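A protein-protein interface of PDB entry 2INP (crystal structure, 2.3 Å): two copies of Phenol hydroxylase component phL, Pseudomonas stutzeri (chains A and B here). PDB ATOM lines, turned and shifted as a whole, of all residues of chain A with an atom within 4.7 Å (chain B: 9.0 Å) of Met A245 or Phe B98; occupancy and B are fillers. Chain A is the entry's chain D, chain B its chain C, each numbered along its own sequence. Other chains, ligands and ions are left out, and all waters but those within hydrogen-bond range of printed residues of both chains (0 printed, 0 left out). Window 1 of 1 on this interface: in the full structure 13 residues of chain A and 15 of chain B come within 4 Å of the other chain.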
ATOM      1  N   SER A  95     -12.234 -18.851 -27.043  1.00  0.00           N
ATOM      2  CA  SER A  95     -12.809 -17.674 -26.444  1.00  0.00           C
ATOM      3  C   SER A  95     -12.717 -16.470 -27.361  1.00  0.00           C
ATOM      4  O   SER A  95     -13.701 -15.715 -27.479  1.00  0.00           O
ATOM      5  CB  SER A  95     -12.024 -17.347 -25.212  1.00  0.00           C
ATOM      6  OG  SER A  95     -12.153 -18.408 -24.293  1.00  0.00           O
ATOM      7  N   PHE A  98     -15.366 -17.212 -30.245  1.00  0.00           N
ATOM      8  CA  PHE A  98     -16.616 -16.817 -29.681  1.00  0.00           C
ATOM      9  C   PHE A  98     -16.799 -15.310 -29.519  1.00  0.00           C
ATOM     10  O   PHE A  98     -17.789 -14.828 -30.042  1.00  0.00           O
ATOM     11  CB  PHE A  98     -16.885 -17.572 -28.387  1.00  0.00           C
ATOM     12  CG  PHE A  98     -18.309 -17.512 -27.948  1.00  0.00           C
ATOM     13  CD1 PHE A  98     -19.250 -18.379 -28.503  1.00  0.00           C
ATOM     14  CD2 PHE A  98     -18.731 -16.546 -27.014  1.00  0.00           C
ATOM     15  CE1 PHE A  98     -20.582 -18.285 -28.129  1.00  0.00           C
ATOM     16  CE2 PHE A  98     -20.036 -16.462 -26.621  1.00  0.00           C
ATOM     17  CZ  PHE A  98     -20.964 -17.346 -27.163  1.00  0.00           C
ATOM     18  N   CYS A  99     -15.902 -14.547 -28.872  1.00  0.00           N
ATOM     19  CA  CYS A  99     -16.146 -13.065 -28.712  1.00  0.00           C
ATOM     20  C   CYS A  99     -16.232 -12.309 -30.010  1.00  0.00           C
ATOM     21  O   CYS A  99     -16.866 -11.279 -30.066  1.00  0.00           O
ATOM     22  CB  CYS A  99     -15.152 -12.303 -27.826  1.00  0.00           C
ATOM     23  SG  CYS A  99     -15.152 -12.953 -26.194  1.00  0.00           S
ATOM     24  N   LEU A 104     -19.137  -9.481 -29.058  1.00  0.00           N
ATOM     25  CA  LEU A 104     -19.213  -9.120 -27.675  1.00  0.00           C
ATOM     26  C   LEU A 104     -18.422  -7.893 -27.325  1.00  0.00           C
ATOM     27  O   LEU A 104     -18.687  -7.244 -26.327  1.00  0.00           O
ATOM     28  CB  LEU A 104     -18.764 -10.288 -26.821  1.00  0.00           C
ATOM     29  CG  LEU A 104     -19.614 -11.544 -26.944  1.00  0.00           C
ATOM     30  CD1 LEU A 104     -19.059 -12.548 -25.892  1.00  0.00           C
ATOM     31  CD2 LEU A 104     -21.118 -11.312 -26.759  1.00  0.00           C
ATOM     32  N   ASP A 242     -17.453  -9.224 -20.549  1.00  0.00           N
ATOM     33  CA  ASP A 242     -17.143 -10.171 -21.615  1.00  0.00           C
ATOM     34  C   ASP A 242     -15.661 -10.267 -21.995  1.00  0.00           C
ATOM     35  O   ASP A 242     -15.232 -11.290 -22.543  1.00  0.00           O
ATOM     36  CB  ASP A 242     -18.002  -9.874 -22.829  1.00  0.00           C
ATOM     37  CG  ASP A 242     -19.432 -10.398 -22.676  1.00  0.00           C
ATOM     38  OD1 ASP A 242     -19.627 -11.562 -22.208  1.00  0.00           O
ATOM     39  OD2 ASP A 242     -20.362  -9.641 -23.045  1.00  0.00           O
ATOM     40  N   VAL A 243     -14.878  -9.231 -21.682  1.00  0.00           N
ATOM     41  CA  VAL A 243     -13.438  -9.297 -21.841  1.00  0.00           C
ATOM     42  C   VAL A 243     -12.809 -10.391 -20.998  1.00  0.00           C
ATOM     43  O   VAL A 243     -11.739 -10.934 -21.365  1.00  0.00           O
ATOM     44  CB  VAL A 243     -12.741  -7.983 -21.498  1.00  0.00           C
ATOM     45  CG1 VAL A 243     -11.416  -7.818 -22.299  1.00  0.00           C
ATOM     46  CG2 VAL A 243     -13.637  -6.888 -21.874  1.00  0.00           C
ATOM     47  N   SER A 244     -13.451 -10.743 -19.887  1.00  0.00           N
ATOM     48  CA  SER A 244     -12.901 -11.777 -19.040  1.00  0.00           C
ATOM     49  C   SER A 244     -12.538 -13.098 -19.753  1.00  0.00           C
ATOM     50  O   SER A 244     -11.620 -13.783 -19.336  1.00  0.00           O
ATOM     51  CB  SER A 244     -13.806 -12.060 -17.860  1.00  0.00           C
ATOM     52  OG  SER A 244     -13.842 -10.939 -17.018  1.00  0.00           O
ATOM     53  N   MET A 245     -13.264 -13.471 -20.791  1.00  0.00           N
ATOM     54  CA  MET A 245     -12.995 -14.755 -21.389  1.00  0.00           C
ATOM     55  C   MET A 245     -11.717 -14.642 -22.198  1.00  0.00           C
ATOM     56  O   MET A 245     -11.063 -15.640 -22.435  1.00  0.00           O
ATOM     57  CB  MET A 245     -14.214 -15.346 -22.132  1.00  0.00           C
ATOM     58  CG  MET A 245     -14.602 -14.727 -23.440  1.00  0.00           C
ATOM     59  SD  MET A 245     -16.227 -15.443 -24.051  1.00  0.00           S
ATOM     60  CE  MET A 245     -17.350 -14.442 -23.025  1.00  0.00           C
ATOM     61  N   LEU A 246     -11.335 -13.404 -22.528  1.00  0.00           N
ATOM     62  CA  LEU A 246     -10.110 -13.086 -23.257  1.00  0.00           C
ATOM     63  C   LEU A 246      -8.816 -12.980 -22.394  1.00  0.00           C
ATOM     64  O   LEU A 246      -7.689 -12.897 -22.951  1.00  0.00           O
ATOM     65  CB  LEU A 246     -10.286 -11.794 -24.053  1.00  0.00           C
ATOM     66  CG  LEU A 246     -11.548 -11.730 -24.921  1.00  0.00           C
ATOM     67  CD1 LEU A 246     -11.446 -10.491 -25.907  1.00  0.00           C
ATOM     68  CD2 LEU A 246     -11.790 -13.011 -25.674  1.00  0.00           C
ATOM     69  N   THR A 247      -8.969 -12.952 -21.066  1.00  0.00           N
ATOM     70  CA  THR A 247      -7.849 -12.799 -20.170  1.00  0.00           C
ATOM     71  C   THR A 247      -7.748 -14.040 -19.290  1.00  0.00           C
ATOM     72  O   THR A 247      -6.965 -14.063 -18.353  1.00  0.00           O
ATOM     73  CB  THR A 247      -8.004 -11.517 -19.312  1.00  0.00           C
ATOM     74  OG1 THR A 247      -9.224 -11.623 -18.563  1.00  0.00           O
ATOM     75  CG2 THR A 247      -8.033 -10.242 -20.203  1.00  0.00           C
ATOM     76  N   GLU A 248      -8.486 -15.094 -19.589  1.00  0.00           N
ATOM     77  CA  GLU A 248      -8.295 -16.385 -18.872  1.00  0.00           C
ATOM     78  C   GLU A 248      -6.871 -16.914 -18.937  1.00  0.00           C
ATOM     79  O   GLU A 248      -6.343 -17.393 -17.945  1.00  0.00           O
ATOM     80  CB  GLU A 248      -9.207 -17.495 -19.413  1.00  0.00           C
ATOM     81  CG  GLU A 248     -10.668 -17.375 -19.020  1.00  0.00           C
ATOM     82  CD  GLU A 248     -10.891 -17.598 -17.503  1.00  0.00           C
ATOM     83  OE1 GLU A 248     -11.012 -16.570 -16.799  1.00  0.00           O
ATOM     84  OE2 GLU A 248     -10.897 -18.768 -17.040  1.00  0.00           O
ATOM     85  N   SER B  91     -12.714 -27.624 -26.707  1.00  0.00           N
ATOM     86  CA  SER B  91     -13.450 -26.351 -26.791  1.00  0.00           C
ATOM     87  C   SER B  91     -14.665 -26.269 -25.874  1.00  0.00           C
ATOM     88  O   SER B  91     -14.871 -25.304 -25.205  1.00  0.00           O
ATOM     89  CB  SER B  91     -13.948 -26.106 -28.199  1.00  0.00           C
ATOM     90  OG  SER B  91     -12.905 -25.564 -28.946  1.00  0.00           O
ATOM     91  N   ALA B  92     -15.500 -27.287 -25.890  1.00  0.00           N
ATOM     92  CA  ALA B  92     -16.713 -27.238 -25.108  1.00  0.00           C
ATOM     93  C   ALA B  92     -16.325 -27.186 -23.636  1.00  0.00           C
ATOM     94  O   ALA B  92     -17.025 -26.588 -22.829  1.00  0.00           O
ATOM     95  CB  ALA B  92     -17.618 -28.449 -25.461  1.00  0.00           C
ATOM     96  N   GLU B  93     -15.202 -27.817 -23.301  1.00  0.00           N
ATOM     97  CA  GLU B  93     -14.757 -27.977 -21.933  1.00  0.00           C
ATOM     98  C   GLU B  93     -14.258 -26.627 -21.415  1.00  0.00           C
ATOM     99  O   GLU B  93     -14.496 -26.264 -20.244  1.00  0.00           O
ATOM    100  CB  GLU B  93     -13.675 -29.028 -21.888  1.00  0.00           C
ATOM    101  CG  GLU B  93     -13.597 -29.804 -20.658  1.00  0.00           C
ATOM    102  CD  GLU B  93     -14.917 -30.502 -20.243  1.00  0.00           C
ATOM    103  OE1 GLU B  93     -15.592 -31.234 -21.060  1.00  0.00           O
ATOM    104  OE2 GLU B  93     -15.208 -30.351 -19.035  1.00  0.00           O
ATOM    105  N   THR B  94     -13.664 -25.846 -22.300  1.00  0.00           N
ATOM    106  CA  THR B  94     -13.291 -24.450 -22.046  1.00  0.00           C
ATOM    107  C   THR B  94     -14.504 -23.624 -21.645  1.00  0.00           C
ATOM    108  O   THR B  94     -14.506 -23.023 -20.615  1.00  0.00           O
ATOM    109  CB  THR B  94     -12.614 -23.825 -23.292  1.00  0.00           C
ATOM    110  OG1 THR B  94     -11.428 -24.577 -23.557  1.00  0.00           O
ATOM    111  CG2 THR B  94     -12.282 -22.286 -23.130  1.00  0.00           C
ATOM    112  N   SER B  95     -15.529 -23.665 -22.499  1.00  0.00           N
ATOM    113  CA  SER B  95     -16.816 -23.004 -22.342  1.00  0.00           C
ATOM    114  C   SER B  95     -17.608 -23.334 -21.055  1.00  0.00           C
ATOM    115  O   SER B  95     -18.051 -22.453 -20.350  1.00  0.00           O
ATOM    116  CB  SER B  95     -17.604 -23.322 -23.601  1.00  0.00           C
ATOM    117  OG  SER B  95     -17.032 -22.539 -24.672  1.00  0.00           O
ATOM    118  N   PHE B  96     -17.707 -24.621 -20.761  1.00  0.00           N
ATOM    119  CA  PHE B  96     -18.356 -25.128 -19.576  1.00  0.00           C
ATOM    120  C   PHE B  96     -17.631 -24.765 -18.284  1.00  0.00           C
ATOM    121  O   PHE B  96     -18.294 -24.486 -17.283  1.00  0.00           O
ATOM    122  CB  PHE B  96     -18.497 -26.643 -19.692  1.00  0.00           C
ATOM    123  CG  PHE B  96     -19.814 -27.107 -20.340  1.00  0.00           C
ATOM    124  CD1 PHE B  96     -19.876 -27.432 -21.692  1.00  0.00           C
ATOM    125  CD2 PHE B  96     -20.979 -27.284 -19.559  1.00  0.00           C
ATOM    126  CE1 PHE B  96     -21.071 -27.874 -22.281  1.00  0.00           C
ATOM    127  CE2 PHE B  96     -22.179 -27.719 -20.135  1.00  0.00           C
ATOM    128  CZ  PHE B  96     -22.225 -28.025 -21.507  1.00  0.00           C
ATOM    129  N   GLY B  97     -16.281 -24.757 -18.301  1.00  0.00           N
ATOM    130  CA  GLY B  97     -15.481 -24.486 -17.111  1.00  0.00           C
ATOM    131  C   GLY B  97     -15.680 -23.014 -16.770  1.00  0.00           C
ATOM    132  O   GLY B  97     -15.854 -22.649 -15.620  1.00  0.00           O
ATOM    133  N   PHE B  98     -15.664 -22.186 -17.809  1.00  0.00           N
ATOM    134  CA  PHE B  98     -15.882 -20.799 -17.692  1.00  0.00           C
ATOM    135  C   PHE B  98     -17.280 -20.409 -17.171  1.00  0.00           C
ATOM    136  O   PHE B  98     -17.383 -19.479 -16.397  1.00  0.00           O
ATOM    137  CB  PHE B  98     -15.581 -20.122 -19.018  1.00  0.00           C
ATOM    138  CG  PHE B  98     -15.598 -18.621 -18.941  1.00  0.00           C
ATOM    139  CD1 PHE B  98     -14.542 -17.938 -18.414  1.00  0.00           C
ATOM    140  CD2 PHE B  98     -16.696 -17.904 -19.353  1.00  0.00           C
ATOM    141  CE1 PHE B  98     -14.555 -16.503 -18.331  1.00  0.00           C
ATOM    142  CE2 PHE B  98     -16.737 -16.456 -19.239  1.00  0.00           C
ATOM    143  CZ  PHE B  98     -15.671 -15.769 -18.756  1.00  0.00           C
ATOM    144  N   CYS B  99     -18.339 -21.084 -17.617  1.00  0.00           N
ATOM    145  CA  CYS B  99     -19.698 -20.777 -17.213  1.00  0.00           C
ATOM    146  C   CYS B  99     -19.922 -21.185 -15.772  1.00  0.00           C
ATOM    147  O   CYS B  99     -20.659 -20.538 -15.045  1.00  0.00           O
ATOM    148  CB  CYS B  99     -20.697 -21.574 -18.026  1.00  0.00           C
ATOM    149  SG  CYS B  99     -21.148 -20.817 -19.485  1.00  0.00           S
ATOM    150  N   GLU B 100     -19.321 -22.293 -15.396  1.00  0.00           N
ATOM    151  CA  GLU B 100     -19.394 -22.819 -14.066  1.00  0.00           C
ATOM    152  C   GLU B 100     -18.728 -21.845 -13.063  1.00  0.00           C
ATOM    153  O   GLU B 100     -19.397 -21.369 -12.138  1.00  0.00           O
ATOM    154  CB  GLU B 100     -18.782 -24.210 -14.111  1.00  0.00           C
ATOM    155  CG  GLU B 100     -18.442 -24.837 -12.768  1.00  0.00           C
ATOM    156  CD  GLU B 100     -19.604 -25.610 -12.120  1.00  0.00           C
ATOM    157  OE1 GLU B 100     -19.505 -25.836 -10.881  1.00  0.00           O
ATOM    158  OE2 GLU B 100     -20.596 -26.000 -12.827  1.00  0.00           O
ATOM    159  N   LYS B 101     -17.456 -21.512 -13.298  1.00  0.00           N
ATOM    160  CA  LYS B 101     -16.626 -20.602 -12.502  1.00  0.00           C
ATOM    161  C   LYS B 101     -17.179 -19.211 -12.357  1.00  0.00           C
ATOM    162  O   LYS B 101     -17.047 -18.613 -11.320  1.00  0.00           O
ATOM    163  CB  LYS B 101     -15.289 -20.346 -13.208  1.00  0.00           C
ATOM    164  CG  LYS B 101     -14.209 -21.379 -13.108  1.00  0.00           C
ATOM    165  CD  LYS B 101     -13.079 -21.119 -14.199  1.00  0.00           C
ATOM    166  CE  LYS B 101     -12.397 -19.714 -14.099  1.00  0.00           C
ATOM    167  NZ  LYS B 101     -13.098 -18.432 -14.636  1.00  0.00           N
ATOM    168  N   ARG B 102     -17.663 -18.652 -13.457  1.00  0.00           N
ATOM    169  CA  ARG B 102     -18.197 -17.314 -13.475  1.00  0.00           C
ATOM    170  C   ARG B 102     -19.696 -17.316 -13.098  1.00  0.00           C
ATOM    171  O   ARG B 102     -20.338 -16.277 -13.135  1.00  0.00           O
ATOM    172  CB  ARG B 102     -18.010 -16.640 -14.851  1.00  0.00           C
ATOM    173  CG  ARG B 102     -16.610 -16.384 -15.248  1.00  0.00           C
ATOM    174  CD  ARG B 102     -16.143 -15.030 -14.803  1.00  0.00           C
ATOM    175  NE  ARG B 102     -14.687 -15.011 -14.823  1.00  0.00           N
ATOM    176  CZ  ARG B 102     -13.923 -13.937 -14.650  1.00  0.00           C
ATOM    177  NH1 ARG B 102     -14.446 -12.721 -14.475  1.00  0.00           N
ATOM    178  NH2 ARG B 102     -12.607 -14.084 -14.667  1.00  0.00           N
ATOM    179  N   ASN B 103     -20.251 -18.471 -12.753  1.00  0.00           N
ATOM    180  CA  ASN B 103     -21.664 -18.534 -12.347  1.00  0.00           C
ATOM    181  C   ASN B 103     -22.669 -18.023 -13.374  1.00  0.00           C
ATOM    182  O   ASN B 103     -23.701 -17.427 -13.008  1.00  0.00           O
ATOM    183  CB  ASN B 103     -21.835 -17.751 -11.058  1.00  0.00           C
ATOM    184  CG  ASN B 103     -21.190 -18.439  -9.926  1.00  0.00           C
ATOM    185  OD1 ASN B 103     -21.348 -19.663  -9.766  1.00  0.00           O
ATOM    186  ND2 ASN B 103     -20.397 -17.697  -9.173  1.00  0.00           N
ATOM    187  N   LEU B 104     -22.356 -18.248 -14.660  1.00  0.00           N
ATOM    188  CA  LEU B 104     -23.182 -17.734 -15.721  1.00  0.00           C
ATOM    189  C   LEU B 104     -24.616 -18.297 -15.793  1.00  0.00           C
ATOM    190  O   LEU B 104     -25.514 -17.594 -16.286  1.00  0.00           O
ATOM    191  CB  LEU B 104     -22.439 -17.740 -17.063  1.00  0.00           C
ATOM    192  CG  LEU B 104     -21.156 -16.907 -17.059  1.00  0.00           C
ATOM    193  CD1 LEU B 104     -20.454 -16.980 -18.439  1.00  0.00           C
ATOM    194  CD2 LEU B 104     -21.407 -15.418 -16.599  1.00  0.00           C
ATOM    195  N   LEU B 105     -24.845 -19.502 -15.285  1.00  0.00           N
ATOM    196  CA  LEU B 105     -26.192 -20.110 -15.353  1.00  0.00           C
ATOM    197  C   LEU B 105     -26.860 -20.140 -13.955  1.00  0.00           C
ATOM    198  O   LEU B 105     -28.083 -20.038 -13.857  1.00  0.00           O
ATOM    199  CB  LEU B 105     -26.195 -21.556 -15.941  1.00  0.00           C
ATOM    200  CG  LEU B 105     -25.704 -21.944 -17.351  1.00  0.00           C
ATOM    201  CD1 LEU B 105     -26.379 -23.196 -17.880  1.00  0.00           C
ATOM    202  CD2 LEU B 105     -25.834 -20.832 -18.359  1.00  0.00           C
ATOM    203  N   ARG B 107     -26.584 -17.739 -11.837  1.00  0.00           N
ATOM    204  CA  ARG B 107     -26.983 -16.398 -11.531  1.00  0.00           C
ATOM    205  C   ARG B 107     -28.223 -15.966 -12.299  1.00  0.00           C
ATOM    206  O   ARG B 107     -28.683 -14.834 -12.122  1.00  0.00           O
ATOM    207  CB  ARG B 107     -25.841 -15.395 -11.786  1.00  0.00           C
ATOM    208  CG  ARG B 107     -25.721 -14.945 -13.255  1.00  0.00           C
ATOM    209  CD  ARG B 107     -24.509 -14.013 -13.494  1.00  0.00           C
ATOM    210  NE  ARG B 107     -24.474 -13.669 -14.911  1.00  0.00           N
ATOM    211  CZ  ARG B 107     -23.655 -12.770 -15.467  1.00  0.00           C
ATOM    212  NH1 ARG B 107     -22.758 -12.141 -14.728  1.00  0.00           N
ATOM    213  NH2 ARG B 107     -23.687 -12.559 -16.796  1.00  0.00           N
ATOM    214  N   MET B 170     -25.259 -27.894 -14.219  1.00  0.00           N
ATOM    215  CA  MET B 170     -24.701 -26.629 -13.822  1.00  0.00           C
ATOM    216  C   MET B 170     -25.780 -25.751 -13.064  1.00  0.00           C
ATOM    217  O   MET B 170     -25.524 -25.266 -11.968  1.00  0.00           O
ATOM    218  CB  MET B 170     -24.081 -25.891 -15.003  1.00  0.00           C
ATOM    219  CG  MET B 170     -23.248 -24.709 -14.570  1.00  0.00           C
ATOM    220  SD  MET B 170     -22.521 -23.874 -16.024  1.00  0.00           S
ATOM    221  CE  MET B 170     -21.870 -25.335 -16.864  1.00  0.00           C
ATOM    222  N   GLU B 241     -28.306 -15.532 -23.056  1.00  0.00           N
ATOM    223  CA  GLU B 241     -27.369 -15.620 -24.151  1.00  0.00           C
ATOM    224  C   GLU B 241     -26.132 -16.399 -23.717  1.00  0.00           C
ATOM    225  O   GLU B 241     -25.463 -16.970 -24.562  1.00  0.00           O
ATOM    226  CB  GLU B 241     -26.935 -14.253 -24.653  1.00  0.00           C
ATOM    227  CG  GLU B 241     -26.082 -13.529 -23.658  1.00  0.00           C
ATOM    228  CD  GLU B 241     -25.629 -12.132 -24.109  1.00  0.00           C
ATOM    229  OE1 GLU B 241     -25.176 -11.336 -23.228  1.00  0.00           O
ATOM    230  OE2 GLU B 241     -25.702 -11.852 -25.323  1.00  0.00           O
ATOM    231  N   ASP B 242     -25.812 -16.413 -22.417  1.00  0.00           N
ATOM    232  CA  ASP B 242     -24.562 -17.042 -21.987  1.00  0.00           C
ATOM    233  C   ASP B 242     -24.573 -18.546 -22.211  1.00  0.00           C
ATOM    234  O   ASP B 242     -23.511 -19.170 -22.257  1.00  0.00           O
ATOM    235  CB  ASP B 242     -24.199 -16.698 -20.548  1.00  0.00           C
ATOM    236  CG  ASP B 242     -23.701 -15.266 -20.384  1.00  0.00           C
ATOM    237  OD1 ASP B 242     -23.058 -14.723 -21.330  1.00  0.00           O
ATOM    238  OD2 ASP B 242     -23.956 -14.673 -19.305  1.00  0.00           O
ATOM    239  N   MET B 245     -22.545 -20.309 -25.528  1.00  0.00           N
ATOM    240  CA  MET B 245     -21.196 -20.901 -25.444  1.00  0.00           C
ATOM    241  C   MET B 245     -21.187 -22.400 -25.171  1.00  0.00           C
ATOM    242  O   MET B 245     -20.275 -23.113 -25.604  1.00  0.00           O
ATOM    243  CB  MET B 245     -20.251 -20.086 -24.541  1.00  0.00           C
ATOM    244  CG  MET B 245     -20.346 -20.108 -23.058  1.00  0.00           C
ATOM    245  SD  MET B 245     -19.139 -18.843 -22.252  1.00  0.00           S
ATOM    246  CE  MET B 245     -20.202 -17.372 -22.247  1.00  0.00           C
ATOM    247  N   LEU B 246     -22.242 -22.869 -24.517  1.00  0.00           N
ATOM    248  CA  LEU B 246     -22.375 -24.244 -24.175  1.00  0.00           C
ATOM    249  C   LEU B 246     -22.967 -25.126 -25.320  1.00  0.00           C
ATOM    250  O   LEU B 246     -22.967 -26.363 -25.234  1.00  0.00           O
ATOM    251  CB  LEU B 246     -23.255 -24.375 -22.926  1.00  0.00           C
ATOM    252  CG  LEU B 246     -22.842 -23.640 -21.666  1.00  0.00           C
ATOM    253  CD1 LEU B 246     -23.699 -24.190 -20.508  1.00  0.00           C
ATOM    254  CD2 LEU B 246     -21.399 -23.875 -21.380  1.00  0.00           C
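Among the printed residues, pairs that only touch across the chains: Met A245 with Phe B98, Phe A98 with Met B245 and Glu A248 with Phe B98.
The side-chain hydroxyl of Thr A247 sits at hydrogen-bond distance from the backbone carbonyl oxygen of Ser A244 (3.3 Å). SG of Cys A99 lies close to SD of Met A245 (3.5 Å). The backbone carbonyl oxygen (O) of Met B245 lies close to the side-chain hydroxyl (OG) of Ser B95, at 3.4 Å.
Hydrophobic or aromatic side chains of chain B that line the printed part of chain A: Phe B98 and Met B245. Of the 11 printed residues of chain A, 4 touch a printed residue of chain B. Printed residues of chain A that touch a printed residue of chain B: Phe A98, Ser A244, Met A245 and Glu A248. Hydrophobic or aromatic side chains of chain A that line the printed part of chain B: Phe A98 and Met A245. Along chain A the printed residues that touch a printed residue of chain B span positions 98 to 248. Among the printed residues, 6 pairs touch across the chains.
Phe A98 touches Met B245, and with the chains exchanged Met A245 touches Phe B98. Positions printed for both chains: 95, 98, 99, 104, 242, 245 and 246. Of the 6 pairs that touch across the chains among the printed residues, 2 have their exchanged pair printed and touching as well.
OG of Ser A244 sits at hydrogen-bond distance from NH1 of Arg B102 (3.2 Å). OE1 of Glu A248 is in salt-bridge range of NH2 of Arg B102 (3.6 Å). The side-chain amino group (NZ) of Lys B101 is in salt-bridge range of the side-chain carboxylate (OE2) of Glu A248.
Of the printed residues of chain B, Phe A98 touches Met B245. Of chain B, only Arg B102 (3.2 Å) comes within 4 Å of Ser A244. Met A245 touches one residue of chain B. Leu A246 touches none of the printed residues of chain B. Ser B95 touches none of the printed residues of chain A. Phe B98 touches just these residues of chain A: Met A245 and Glu A248. Printed residues of chain A within 4 Å of Met B245: Phe A98 (3.7 Å). The nearest residue of chain A that does not touch Phe B98 is Ser A244 (4.1 Å).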
